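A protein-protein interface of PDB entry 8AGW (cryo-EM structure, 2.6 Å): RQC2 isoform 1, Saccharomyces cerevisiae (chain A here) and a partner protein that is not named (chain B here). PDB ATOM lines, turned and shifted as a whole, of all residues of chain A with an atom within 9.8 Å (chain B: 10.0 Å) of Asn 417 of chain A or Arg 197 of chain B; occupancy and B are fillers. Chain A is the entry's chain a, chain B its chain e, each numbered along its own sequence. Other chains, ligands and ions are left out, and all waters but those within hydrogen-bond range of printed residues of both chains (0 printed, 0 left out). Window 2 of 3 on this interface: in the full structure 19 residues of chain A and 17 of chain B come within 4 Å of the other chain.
Hydrophobic or aromatic side chains of chain A that line the printed part of chain B: Leu 422. Printed residues of chain B that touch a printed residue of chain A: Tyr 29, Phe 30, Asp 31, Asp 191, Glu 196 and Arg 197. Hydrophobic or aromatic side chains of chain B that line the printed part of chain A: Tyr 29 and Phe 30. Among the printed residues, 10 pairs touch across the chains.
Among the printed residues, merely in contact across the chains: Thr 418 of chain A with Tyr 29 of chain B, Thr 418 of chain A with Phe 30 of chain B, Thr 418 of chain A with Arg 197 of chain B, Lys 421 of chain A with Asp 191 of chain B, Lys 421 of chain A with Glu 196 of chain B, Leu 422 of chain A with Asp 31 of chain B and Ser 425 of chain A with Phe 30 of chain B.
The guanidinium group (NH2) of Arg 197 of chain B lies within salt-bridge range of the side-chain carboxylate (OD2) of Asp 415 of chain A (2.7 Å). OD1 of Asn 417 of chain A sits close to NE of Arg 197 of chain B. The side-chain amino group (NZ) of Lys 421 of chain A lies within hydrogen-bond range of the side-chain hydroxyl (OH) of Tyr 29 of chain B (2.8 Å).
The side-chain hydroxyl (OG1) of Thr 418 of chain A lies within hydrogen-bond range of the backbone carbonyl oxygen (O) of Asp 415 of chain A (2.4 Å). The side-chain carboxylate (OD1) of Asp 195 of chain B lies within hydrogen-bond range of the side-chain hydroxyl (OH) of Tyr 29 of chain B. The side-chain carboxylate of Asp 195 of chain B lies within salt-bridge range of the guanidinium group of Arg 197 of chain B (2.7 Å). NH1 of Arg 197 of chain B lies within hydrogen-bond range of OH of Tyr 198 of chain B (3.3 Å).
Asn 417 of chain A touches one residue of chain B. Arg 197 of chain B touches three residues of chain A. Asp 415 of chain A touches one residue of chain B. Thr 418 of chain A touches three residues of chain B. No residue of chain B comes within 4 Å of Glu 420 of chain A. No residue of chain A comes within 4 Å of Asp 195 of chain B. Glu 196 of chain B touches just one residue of chain A: Lys 421 (3.6 Å). No residue of chain A comes within 4 Å of Tyr 198 of chain B. Printed residues of chain B within 4 Å of Leu 422 of chain A: Asp 31. Printed residues of chain B within 4 Å of Ser 425 of chain A: Phe 30. Ser 204 of chain B touches none of the printed residues of chain A. Glu 190 of chain B touches none of the printed residues of chain A. The nearest residue of chain B that does not touch Asn 417 of chain A is Tyr 29 of chain B (5.5 Å). The nearest residue of chain A that does not touch Arg 197 of chain B is Trp 416 of chain A (6.4 Å). The nearest printed residue of chain A that does not touch Tyr 29 of chain B is Asn 417 of chain A (5.5 Å).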
ATOM      1  N   ILE A 410      11.666  19.410 -12.502  1.00  0.00           N
ATOM      2  CA  ILE A 410      12.479  20.571 -12.864  1.00  0.00           C
ATOM      3  C   ILE A 410      13.941  20.178 -13.042  1.00  0.00           C
ATOM      4  O   ILE A 410      14.603  20.603 -13.997  1.00  0.00           O
ATOM      5  CB  ILE A 410      12.296  21.689 -11.819  1.00  0.00           C
ATOM      6  CG1 ILE A 410      10.948  22.380 -12.023  1.00  0.00           C
ATOM      7  CG2 ILE A 410      13.432  22.697 -11.844  1.00  0.00           C
ATOM      8  CD1 ILE A 410      10.678  23.491 -11.044  1.00  0.00           C
ATOM      9  N   GLN A 413      15.690  19.170 -16.280  1.00  0.00           N
ATOM     10  CA  GLN A 413      15.799  20.249 -17.270  1.00  0.00           C
ATOM     11  C   GLN A 413      14.704  20.142 -18.326  1.00  0.00           C
ATOM     12  O   GLN A 413      14.945  20.315 -19.521  1.00  0.00           O
ATOM     13  CB  GLN A 413      17.186  20.291 -17.915  1.00  0.00           C
ATOM     14  CG  GLN A 413      18.225  21.004 -17.085  1.00  0.00           C
ATOM     15  CD  GLN A 413      19.495  21.252 -17.861  1.00  0.00           C
ATOM     16  OE1 GLN A 413      20.494  20.562 -17.671  1.00  0.00           O
ATOM     17  NE2 GLN A 413      19.459  22.233 -18.752  1.00  0.00           N
ATOM     18  N   MET A 414      13.496  19.828 -17.877  1.00  0.00           N
ATOM     19  CA  MET A 414      12.387  19.605 -18.783  1.00  0.00           C
ATOM     20  C   MET A 414      11.695  20.932 -19.073  1.00  0.00           C
ATOM     21  O   MET A 414      11.685  21.842 -18.241  1.00  0.00           O
ATOM     22  CB  MET A 414      11.425  18.584 -18.170  1.00  0.00           C
ATOM     23  CG  MET A 414      10.266  18.131 -19.039  1.00  0.00           C
ATOM     24  SD  MET A 414       9.232  16.924 -18.197  1.00  0.00           S
ATOM     25  CE  MET A 414      10.321  15.502 -18.222  1.00  0.00           C
ATOM     26  N   ASP A 415      11.138  21.040 -20.278  1.00  0.00           N
ATOM     27  CA  ASP A 415      10.454  22.248 -20.708  1.00  0.00           C
ATOM     28  C   ASP A 415       9.201  22.480 -19.871  1.00  0.00           C
ATOM     29  O   ASP A 415       8.489  21.542 -19.509  1.00  0.00           O
ATOM     30  CB  ASP A 415      10.089  22.140 -22.188  1.00  0.00           C
ATOM     31  CG  ASP A 415       9.503  23.418 -22.744  1.00  0.00           C
ATOM     32  OD1 ASP A 415       9.733  24.494 -22.154  1.00  0.00           O
ATOM     33  OD2 ASP A 415       8.803  23.347 -23.772  1.00  0.00           O
ATOM     34  N   TRP A 416       8.947  23.758 -19.558  1.00  0.00           N
ATOM     35  CA  TRP A 416       7.888  24.115 -18.618  1.00  0.00           C
ATOM     36  C   TRP A 416       6.503  23.798 -19.166  1.00  0.00           C
ATOM     37  O   TRP A 416       5.625  23.344 -18.421  1.00  0.00           O
ATOM     38  CB  TRP A 416       7.986  25.600 -18.261  1.00  0.00           C
ATOM     39  CG  TRP A 416       9.186  25.953 -17.435  1.00  0.00           C
ATOM     40  CD1 TRP A 416      10.088  25.089 -16.894  1.00  0.00           C
ATOM     41  CD2 TRP A 416       9.597  27.264 -17.029  1.00  0.00           C
ATOM     42  NE1 TRP A 416      11.044  25.777 -16.191  1.00  0.00           N
ATOM     43  CE2 TRP A 416      10.764  27.115 -16.257  1.00  0.00           C
ATOM     44  CE3 TRP A 416       9.095  28.549 -17.249  1.00  0.00           C
ATOM     45  CZ2 TRP A 416      11.434  28.199 -15.703  1.00  0.00           C
ATOM     46  CZ3 TRP A 416       9.763  29.624 -16.694  1.00  0.00           C
ATOM     47  CH2 TRP A 416      10.920  29.442 -15.934  1.00  0.00           C
ATOM     48  N   ASN A 417       6.299  23.994 -20.467  1.00  0.00           N
ATOM     49  CA  ASN A 417       5.001  23.704 -21.059  1.00  0.00           C
ATOM     50  C   ASN A 417       4.767  22.203 -21.148  1.00  0.00           C
ATOM     51  O   ASN A 417       3.640  21.734 -20.964  1.00  0.00           O
ATOM     52  CB  ASN A 417       4.901  24.357 -22.431  1.00  0.00           C
ATOM     53  CG  ASN A 417       4.831  25.864 -22.345  1.00  0.00           C
ATOM     54  OD1 ASN A 417       5.584  26.571 -23.008  1.00  0.00           O
ATOM     55  ND2 ASN A 417       3.940  26.364 -21.500  1.00  0.00           N
ATOM     56  N   THR A 418       5.829  21.434 -21.402  1.00  0.00           N
ATOM     57  CA  THR A 418       5.717  19.982 -21.346  1.00  0.00           C
ATOM     58  C   THR A 418       5.453  19.490 -19.931  1.00  0.00           C
ATOM     59  O   THR A 418       4.733  18.501 -19.757  1.00  0.00           O
ATOM     60  CB  THR A 418       6.987  19.329 -21.882  1.00  0.00           C
ATOM     61  OG1 THR A 418       8.095  19.716 -21.066  1.00  0.00           O
ATOM     62  CG2 THR A 418       7.252  19.782 -23.299  1.00  0.00           C
ATOM     63  N   ILE A 419       5.988  20.176 -18.920  1.00  0.00           N
ATOM     64  CA  ILE A 419       5.662  19.841 -17.536  1.00  0.00           C
ATOM     65  C   ILE A 419       4.191  20.120 -17.245  1.00  0.00           C
ATOM     66  O   ILE A 419       3.517  19.294 -16.616  1.00  0.00           O
ATOM     67  CB  ILE A 419       6.595  20.596 -16.570  1.00  0.00           C
ATOM     68  CG1 ILE A 419       8.013  20.032 -16.654  1.00  0.00           C
ATOM     69  CG2 ILE A 419       6.104  20.519 -15.132  1.00  0.00           C
ATOM     70  CD1 ILE A 419       9.008  20.727 -15.745  1.00  0.00           C
ATOM     71  N   GLU A 420       3.662  21.244 -17.734  1.00  0.00           N
ATOM     72  CA  GLU A 420       2.241  21.540 -17.544  1.00  0.00           C
ATOM     73  C   GLU A 420       1.348  20.543 -18.277  1.00  0.00           C
ATOM     74  O   GLU A 420       0.286  20.161 -17.767  1.00  0.00           O
ATOM     75  CB  GLU A 420       1.933  22.969 -17.988  1.00  0.00           C
ATOM     76  CG  GLU A 420       2.480  24.035 -17.053  1.00  0.00           C
ATOM     77  CD  GLU A 420       2.617  25.388 -17.719  1.00  0.00           C
ATOM     78  OE1 GLU A 420       1.720  25.760 -18.502  1.00  0.00           O
ATOM     79  OE2 GLU A 420       3.614  26.089 -17.446  1.00  0.00           O
ATOM     80  N   LYS A 421       1.767  20.093 -19.463  1.00  0.00           N
ATOM     81  CA  LYS A 421       1.000  19.078 -20.182  1.00  0.00           C
ATOM     82  C   LYS A 421       1.048  17.737 -19.459  1.00  0.00           C
ATOM     83  O   LYS A 421       0.055  16.994 -19.441  1.00  0.00           O
ATOM     84  CB  LYS A 421       1.519  18.943 -21.613  1.00  0.00           C
ATOM     85  CG  LYS A 421       1.236  20.160 -22.478  1.00  0.00           C
ATOM     86  CD  LYS A 421      -0.244  20.330 -22.761  1.00  0.00           C
ATOM     87  CE  LYS A 421      -0.820  19.112 -23.453  1.00  0.00           C
ATOM     88  NZ  LYS A 421      -0.200  18.939 -24.793  1.00  0.00           N
ATOM     89  N   LEU A 422       2.188  17.422 -18.841  1.00  0.00           N
ATOM     90  CA  LEU A 422       2.286  16.244 -17.990  1.00  0.00           C
ATOM     91  C   LEU A 422       1.396  16.346 -16.758  1.00  0.00           C
ATOM     92  O   LEU A 422       0.860  15.327 -16.311  1.00  0.00           O
ATOM     93  CB  LEU A 422       3.741  16.033 -17.575  1.00  0.00           C
ATOM     94  CG  LEU A 422       4.062  14.787 -16.751  1.00  0.00           C
ATOM     95  CD1 LEU A 422       3.645  13.544 -17.498  1.00  0.00           C
ATOM     96  CD2 LEU A 422       5.531  14.733 -16.421  1.00  0.00           C
ATOM     97  N   ILE A 423       1.223  17.545 -16.209  1.00  0.00           N
ATOM     98  CA  ILE A 423       0.309  17.716 -15.084  1.00  0.00           C
ATOM     99  C   ILE A 423      -1.138  17.519 -15.530  1.00  0.00           C
ATOM    100  O   ILE A 423      -1.919  16.851 -14.843  1.00  0.00           O
ATOM    101  CB  ILE A 423       0.520  19.086 -14.409  1.00  0.00           C
ATOM    102  CG1 ILE A 423       1.923  19.172 -13.815  1.00  0.00           C
ATOM    103  CG2 ILE A 423      -0.485  19.313 -13.292  1.00  0.00           C
ATOM    104  CD1 ILE A 423       2.203  18.130 -12.766  1.00  0.00           C
ATOM    105  N   LYS A 424      -1.498  18.065 -16.701  1.00  0.00           N
ATOM    106  CA  LYS A 424      -2.857  17.897 -17.226  1.00  0.00           C
ATOM    107  C   LYS A 424      -3.184  16.437 -17.512  1.00  0.00           C
ATOM    108  O   LYS A 424      -4.283  15.964 -17.188  1.00  0.00           O
ATOM    109  CB  LYS A 424      -3.056  18.716 -18.502  1.00  0.00           C
ATOM    110  CG  LYS A 424      -2.944  20.201 -18.326  1.00  0.00           C
ATOM    111  CD  LYS A 424      -3.303  20.952 -19.588  1.00  0.00           C
ATOM    112  CE  LYS A 424      -2.927  22.418 -19.467  1.00  0.00           C
ATOM    113  NZ  LYS A 424      -3.266  23.186 -20.694  1.00  0.00           N
ATOM    114  N   SER A 425      -2.238  15.705 -18.109  1.00  0.00           N
ATOM    115  CA  SER A 425      -2.488  14.305 -18.437  1.00  0.00           C
ATOM    116  C   SER A 425      -2.622  13.449 -17.185  1.00  0.00           C
ATOM    117  O   SER A 425      -3.477  12.561 -17.124  1.00  0.00           O
ATOM    118  CB  SER A 425      -1.376  13.772 -19.330  1.00  0.00           C
ATOM    119  OG  SER A 425      -1.382  12.358 -19.362  1.00  0.00           O
ATOM    120  N   LEU A 439      -3.067  24.760 -12.710  1.00  0.00           N
ATOM    121  CA  LEU A 439      -2.247  24.720 -13.918  1.00  0.00           C
ATOM    122  C   LEU A 439      -1.496  25.995 -14.325  1.00  0.00           C
ATOM    123  O   LEU A 439      -0.404  25.840 -14.898  1.00  0.00           O
ATOM    124  CB  LEU A 439      -3.103  24.222 -15.083  1.00  0.00           C
ATOM    125  CG  LEU A 439      -3.167  22.718 -14.839  1.00  0.00           C
ATOM    126  CD1 LEU A 439      -4.470  22.079 -15.319  1.00  0.00           C
ATOM    127  CD2 LEU A 439      -1.919  22.047 -15.384  1.00  0.00           C
ATOM    128  N   PRO A 440      -1.984  27.256 -14.118  1.00  0.00           N
ATOM    129  CA  PRO A 440      -1.117  28.393 -14.471  1.00  0.00           C
ATOM    130  C   PRO A 440       0.083  28.534 -13.546  1.00  0.00           C
ATOM    131  O   PRO A 440       0.055  29.284 -12.566  1.00  0.00           O
ATOM    132  CB  PRO A 440      -2.051  29.606 -14.382  1.00  0.00           C
ATOM    133  CG  PRO A 440      -3.176  29.176 -13.550  1.00  0.00           C
ATOM    134  CD  PRO A 440      -3.357  27.725 -13.838  1.00  0.00           C
ATOM    135  N   LEU A 441       1.144  27.804 -13.874  1.00  0.00           N
ATOM    136  CA  LEU A 441       2.309  27.683 -13.012  1.00  0.00           C
ATOM    137  C   LEU A 441       3.238  28.882 -13.161  1.00  0.00           C
ATOM    138  O   LEU A 441       3.582  29.297 -14.271  1.00  0.00           O
ATOM    139  CB  LEU A 441       3.073  26.403 -13.344  1.00  0.00           C
ATOM    140  CG  LEU A 441       2.677  25.174 -12.532  1.00  0.00           C
ATOM    141  CD1 LEU A 441       3.457  23.955 -12.996  1.00  0.00           C
ATOM    142  CD2 LEU A 441       2.873  25.425 -11.055  1.00  0.00           C
ATOM    143  N   LEU A 443       6.513  29.205 -12.720  1.00  0.00           N
ATOM    144  CA  LEU A 443       7.878  28.701 -12.610  1.00  0.00           C
ATOM    145  C   LEU A 443       8.920  29.773 -12.885  1.00  0.00           C
ATOM    146  O   LEU A 443      10.092  29.581 -12.544  1.00  0.00           O
ATOM    147  CB  LEU A 443       8.080  27.525 -13.563  1.00  0.00           C
ATOM    148  CG  LEU A 443       7.140  26.336 -13.376  1.00  0.00           C
ATOM    149  CD1 LEU A 443       7.607  25.166 -14.216  1.00  0.00           C
ATOM    150  CD2 LEU A 443       7.072  25.936 -11.911  1.00  0.00           C
ATOM    151  N   TYR B  29       4.593  12.950 -26.439  1.00  0.00           N
ATOM    152  CA  TYR B  29       5.870  13.597 -26.179  1.00  0.00           C
ATOM    153  C   TYR B  29       6.174  13.841 -24.719  1.00  0.00           C
ATOM    154  O   TYR B  29       7.306  13.676 -24.294  1.00  0.00           O
ATOM    155  CB  TYR B  29       5.987  14.897 -26.983  1.00  0.00           C
ATOM    156  CG  TYR B  29       5.044  16.016 -26.609  1.00  0.00           C
ATOM    157  CD1 TYR B  29       3.755  16.056 -27.101  1.00  0.00           C
ATOM    158  CD2 TYR B  29       5.464  17.056 -25.798  1.00  0.00           C
ATOM    159  CE1 TYR B  29       2.895  17.081 -26.770  1.00  0.00           C
ATOM    160  CE2 TYR B  29       4.613  18.085 -25.462  1.00  0.00           C
ATOM    161  CZ  TYR B  29       3.331  18.091 -25.952  1.00  0.00           C
ATOM    162  OH  TYR B  29       2.486  19.119 -25.624  1.00  0.00           O
ATOM    163  N   PHE B  30       5.180  14.238 -23.945  1.00  0.00           N
ATOM    164  CA  PHE B  30       5.425  14.580 -22.549  1.00  0.00           C
ATOM    165  C   PHE B  30       5.912  13.462 -21.639  1.00  0.00           C
ATOM    166  O   PHE B  30       6.741  13.702 -20.771  1.00  0.00           O
ATOM    167  CB  PHE B  30       4.249  15.342 -21.921  1.00  0.00           C
ATOM    168  CG  PHE B  30       2.899  14.862 -22.343  1.00  0.00           C
ATOM    169  CD1 PHE B  30       2.279  15.397 -23.455  1.00  0.00           C
ATOM    170  CD2 PHE B  30       2.232  13.914 -21.601  1.00  0.00           C
ATOM    171  CE1 PHE B  30       1.030  14.968 -23.838  1.00  0.00           C
ATOM    172  CE2 PHE B  30       0.981  13.480 -21.978  1.00  0.00           C
ATOM    173  CZ  PHE B  30       0.378  14.008 -23.097  1.00  0.00           C
ATOM    174  N   ASP B  31       5.413  12.249 -21.810  1.00  0.00           N
ATOM    175  CA  ASP B  31       5.779  11.182 -20.889  1.00  0.00           C
ATOM    176  C   ASP B  31       6.305   9.947 -21.565  1.00  0.00           C
ATOM    177  O   ASP B  31       6.129   9.775 -22.759  1.00  0.00           O
ATOM    178  CB  ASP B  31       4.635  10.834 -19.926  1.00  0.00           C
ATOM    179  CG  ASP B  31       3.430  10.223 -20.616  1.00  0.00           C
ATOM    180  OD1 ASP B  31       3.529   9.103 -21.153  1.00  0.00           O
ATOM    181  OD2 ASP B  31       2.353  10.846 -20.576  1.00  0.00           O
ATOM    182  N   ARG B  57      15.298  18.280 -29.807  1.00  0.00           N
ATOM    183  CA  ARG B  57      14.285  18.425 -30.858  1.00  0.00           C
ATOM    184  C   ARG B  57      14.739  18.473 -32.291  1.00  0.00           C
ATOM    185  O   ARG B  57      14.084  17.915 -33.161  1.00  0.00           O
ATOM    186  CB  ARG B  57      13.479  19.687 -30.611  1.00  0.00           C
ATOM    187  CG  ARG B  57      12.610  19.659 -29.369  1.00  0.00           C
ATOM    188  CD  ARG B  57      11.550  20.750 -29.417  1.00  0.00           C
ATOM    189  NE  ARG B  57      10.647  20.583 -30.554  1.00  0.00           N
ATOM    190  CZ  ARG B  57      10.694  21.307 -31.670  1.00  0.00           C
ATOM    191  NH1 ARG B  57      11.595  22.270 -31.805  1.00  0.00           N
ATOM    192  NH2 ARG B  57       9.833  21.069 -32.649  1.00  0.00           N
ATOM    193  N   GLU B 190      -4.906  14.276 -30.705  1.00  0.00           N
ATOM    194  CA  GLU B 190      -3.971  14.924 -31.608  1.00  0.00           C
ATOM    195  C   GLU B 190      -2.970  15.754 -30.842  1.00  0.00           C
ATOM    196  O   GLU B 190      -1.785  15.765 -31.169  1.00  0.00           O
ATOM    197  CB  GLU B 190      -4.717  15.837 -32.571  1.00  0.00           C
ATOM    198  CG  GLU B 190      -5.756  15.130 -33.424  1.00  0.00           C
ATOM    199  CD  GLU B 190      -7.142  15.186 -32.819  1.00  0.00           C
ATOM    200  OE1 GLU B 190      -7.350  15.978 -31.875  1.00  0.00           O
ATOM    201  OE2 GLU B 190      -8.026  14.439 -33.287  1.00  0.00           O
ATOM    202  N   ASP B 191      -3.435  16.453 -29.819  1.00  0.00           N
ATOM    203  CA  ASP B 191      -2.555  17.282 -29.012  1.00  0.00           C
ATOM    204  C   ASP B 191      -1.494  16.481 -28.292  1.00  0.00           C
ATOM    205  O   ASP B 191      -0.353  16.906 -28.193  1.00  0.00           O
ATOM    206  CB  ASP B 191      -3.368  18.044 -27.982  1.00  0.00           C
ATOM    207  CG  ASP B 191      -4.383  18.969 -28.615  1.00  0.00           C
ATOM    208  OD1 ASP B 191      -4.319  19.173 -29.844  1.00  0.00           O
ATOM    209  OD2 ASP B 191      -5.245  19.495 -27.881  1.00  0.00           O
ATOM    210  N   ILE B 193      -0.121  13.655 -29.159  1.00  0.00           N
ATOM    211  CA  ILE B 193       0.893  13.186 -30.094  1.00  0.00           C
ATOM    212  C   ILE B 193       1.880  14.256 -30.520  1.00  0.00           C
ATOM    213  O   ILE B 193       3.080  14.011 -30.566  1.00  0.00           O
ATOM    214  CB  ILE B 193       0.244  12.569 -31.347  1.00  0.00           C
ATOM    215  CG1 ILE B 193      -0.610  11.362 -30.966  1.00  0.00           C
ATOM    216  CG2 ILE B 193       1.286  12.148 -32.368  1.00  0.00           C
ATOM    217  CD1 ILE B 193       0.203  10.158 -30.553  1.00  0.00           C
ATOM    218  N   SER B 194       1.397  15.457 -30.802  1.00  0.00           N
ATOM    219  CA  SER B 194       2.278  16.502 -31.315  1.00  0.00           C
ATOM    220  C   SER B 194       2.198  17.785 -30.521  1.00  0.00           C
ATOM    221  O   SER B 194       1.114  18.243 -30.192  1.00  0.00           O
ATOM    222  CB  SER B 194       1.911  16.820 -32.758  1.00  0.00           C
ATOM    223  OG  SER B 194       1.574  15.649 -33.477  1.00  0.00           O
ATOM    224  N   ASP B 195       3.340  18.396 -30.245  1.00  0.00           N
ATOM    225  CA  ASP B 195       3.346  19.608 -29.441  1.00  0.00           C
ATOM    226  C   ASP B 195       2.635  20.751 -30.121  1.00  0.00           C
ATOM    227  O   ASP B 195       2.895  21.052 -31.281  1.00  0.00           O
ATOM    228  CB  ASP B 195       4.777  20.020 -29.134  1.00  0.00           C
ATOM    229  CG  ASP B 195       4.873  20.989 -27.977  1.00  0.00           C
ATOM    230  OD1 ASP B 195       3.847  21.269 -27.325  1.00  0.00           O
ATOM    231  OD2 ASP B 195       5.991  21.463 -27.711  1.00  0.00           O
ATOM    232  N   GLU B 196       1.762  21.421 -29.387  1.00  0.00           N
ATOM    233  CA  GLU B 196       1.016  22.545 -29.932  1.00  0.00           C
ATOM    234  C   GLU B 196       1.866  23.731 -30.315  1.00  0.00           C
ATOM    235  O   GLU B 196       1.598  24.393 -31.300  1.00  0.00           O
ATOM    236  CB  GLU B 196      -0.045  22.977 -28.931  1.00  0.00           C
ATOM    237  CG  GLU B 196       0.412  22.885 -27.486  1.00  0.00           C
ATOM    238  CD  GLU B 196      -0.731  23.038 -26.507  1.00  0.00           C
ATOM    239  OE1 GLU B 196      -1.875  23.243 -26.960  1.00  0.00           O
ATOM    240  OE2 GLU B 196      -0.486  22.951 -25.287  1.00  0.00           O
ATOM    241  N   ARG B 197       2.877  24.032 -29.523  1.00  0.00           N
ATOM    242  CA  ARG B 197       3.671  25.217 -29.790  1.00  0.00           C
ATOM    243  C   ARG B 197       4.359  25.142 -31.126  1.00  0.00           C
ATOM    244  O   ARG B 197       4.461  26.136 -31.833  1.00  0.00           O
ATOM    245  CB  ARG B 197       4.690  25.430 -28.677  1.00  0.00           C
ATOM    246  CG  ARG B 197       4.077  26.061 -27.443  1.00  0.00           C
ATOM    247  CD  ARG B 197       5.037  26.055 -26.269  1.00  0.00           C
ATOM    248  NE  ARG B 197       5.409  24.699 -25.895  1.00  0.00           N
ATOM    249  CZ  ARG B 197       6.644  24.218 -25.965  1.00  0.00           C
ATOM    250  NH1 ARG B 197       7.637  24.991 -26.377  1.00  0.00           N
ATOM    251  NH2 ARG B 197       6.884  22.968 -25.608  1.00  0.00           N
ATOM    252  N   TYR B 198       4.849  23.971 -31.475  1.00  0.00           N
ATOM    253  CA  TYR B 198       5.581  23.843 -32.711  1.00  0.00           C
ATOM    254  C   TYR B 198       4.737  23.364 -33.881  1.00  0.00           C
ATOM    255  O   TYR B 198       5.257  23.175 -34.975  1.00  0.00           O
ATOM    256  CB  TYR B 198       6.795  22.958 -32.498  1.00  0.00           C
ATOM    257  CG  TYR B 198       7.713  23.485 -31.427  1.00  0.00           C
ATOM    258  CD1 TYR B 198       8.539  24.569 -31.673  1.00  0.00           C
ATOM    259  CD2 TYR B 198       7.751  22.906 -30.170  1.00  0.00           C
ATOM    260  CE1 TYR B 198       9.380  25.062 -30.697  1.00  0.00           C
ATOM    261  CE2 TYR B 198       8.590  23.390 -29.187  1.00  0.00           C
ATOM    262  CZ  TYR B 198       9.402  24.467 -29.456  1.00  0.00           C
ATOM    263  OH  TYR B 198      10.241  24.957 -28.484  1.00  0.00           O
ATOM    264  N   SER B 199       3.441  23.170 -33.666  1.00  0.00           N
ATOM    265  CA  SER B 199       2.563  22.773 -34.766  1.00  0.00           C
ATOM    266  C   SER B 199       1.222  23.494 -34.818  1.00  0.00           C
ATOM    267  O   SER B 199       0.709  23.939 -33.803  1.00  0.00           O
ATOM    268  CB  SER B 199       2.334  21.267 -34.754  1.00  0.00           C
ATOM    269  OG  SER B 199       1.469  20.875 -35.804  1.00  0.00           O
ATOM    270  N   SER B 200       0.636  23.592 -36.002  1.00  0.00           N
ATOM    271  CA  SER B 200      -0.647  24.267 -36.164  1.00  0.00           C
ATOM    272  C   SER B 200      -1.815  23.377 -35.779  1.00  0.00           C
ATOM    273  O   SER B 200      -1.611  22.241 -35.366  1.00  0.00           O
ATOM    274  CB  SER B 200      -0.805  24.755 -37.594  1.00  0.00           C
ATOM    275  OG  SER B 200      -0.436  23.746 -38.511  1.00  0.00           O
ATOM    276  N   LYS B 201      -3.034  23.899 -35.840  1.00  0.00           N
ATOM    277  CA  LYS B 201      -4.198  23.065 -35.564  1.00  0.00           C
ATOM    278  C   LYS B 201      -4.223  21.984 -36.608  1.00  0.00           C
ATOM    279  O   LYS B 201      -4.462  20.825 -36.301  1.00  0.00           O
ATOM    280  CB  LYS B 201      -5.473  23.888 -35.640  1.00  0.00           C
ATOM    281  CG  LYS B 201      -6.654  23.245 -34.936  1.00  0.00           C
ATOM    282  CD  LYS B 201      -6.284  22.887 -33.506  1.00  0.00           C
ATOM    283  CE  LYS B 201      -7.470  22.317 -32.748  1.00  0.00           C
ATOM    284  NZ  LYS B 201      -8.010  21.089 -33.391  1.00  0.00           N
ATOM    285  N   GLU B 202      -3.958  22.350 -37.852  1.00  0.00           N
ATOM    286  CA  GLU B 202      -3.846  21.348 -38.895  1.00  0.00           C
ATOM    287  C   GLU B 202      -2.446  20.837 -38.724  1.00  0.00           C
ATOM    288  O   GLU B 202      -1.722  21.391 -37.921  1.00  0.00           O
ATOM    289  CB  GLU B 202      -4.056  21.942 -40.283  1.00  0.00           C
ATOM    290  CG  GLU B 202      -2.952  22.868 -40.772  1.00  0.00           C
ATOM    291  CD  GLU B 202      -3.200  24.325 -40.434  1.00  0.00           C
ATOM    292  OE1 GLU B 202      -4.226  24.629 -39.789  1.00  0.00           O
ATOM    293  OE2 GLU B 202      -2.364  25.169 -40.817  1.00  0.00           O
ATOM    294  N   SER B 204      -1.202  18.871 -36.879  1.00  0.00           N
ATOM    295  CA  SER B 204      -1.382  18.056 -35.700  1.00  0.00           C
ATOM    296  C   SER B 204      -2.470  17.074 -36.017  1.00  0.00           C
ATOM    297  O   SER B 204      -2.356  15.890 -35.709  1.00  0.00           O
ATOM    298  CB  SER B 204      -1.805  18.911 -34.522  1.00  0.00           C
ATOM    299  OG  SER B 204      -0.779  19.805 -34.143  1.00  0.00           O
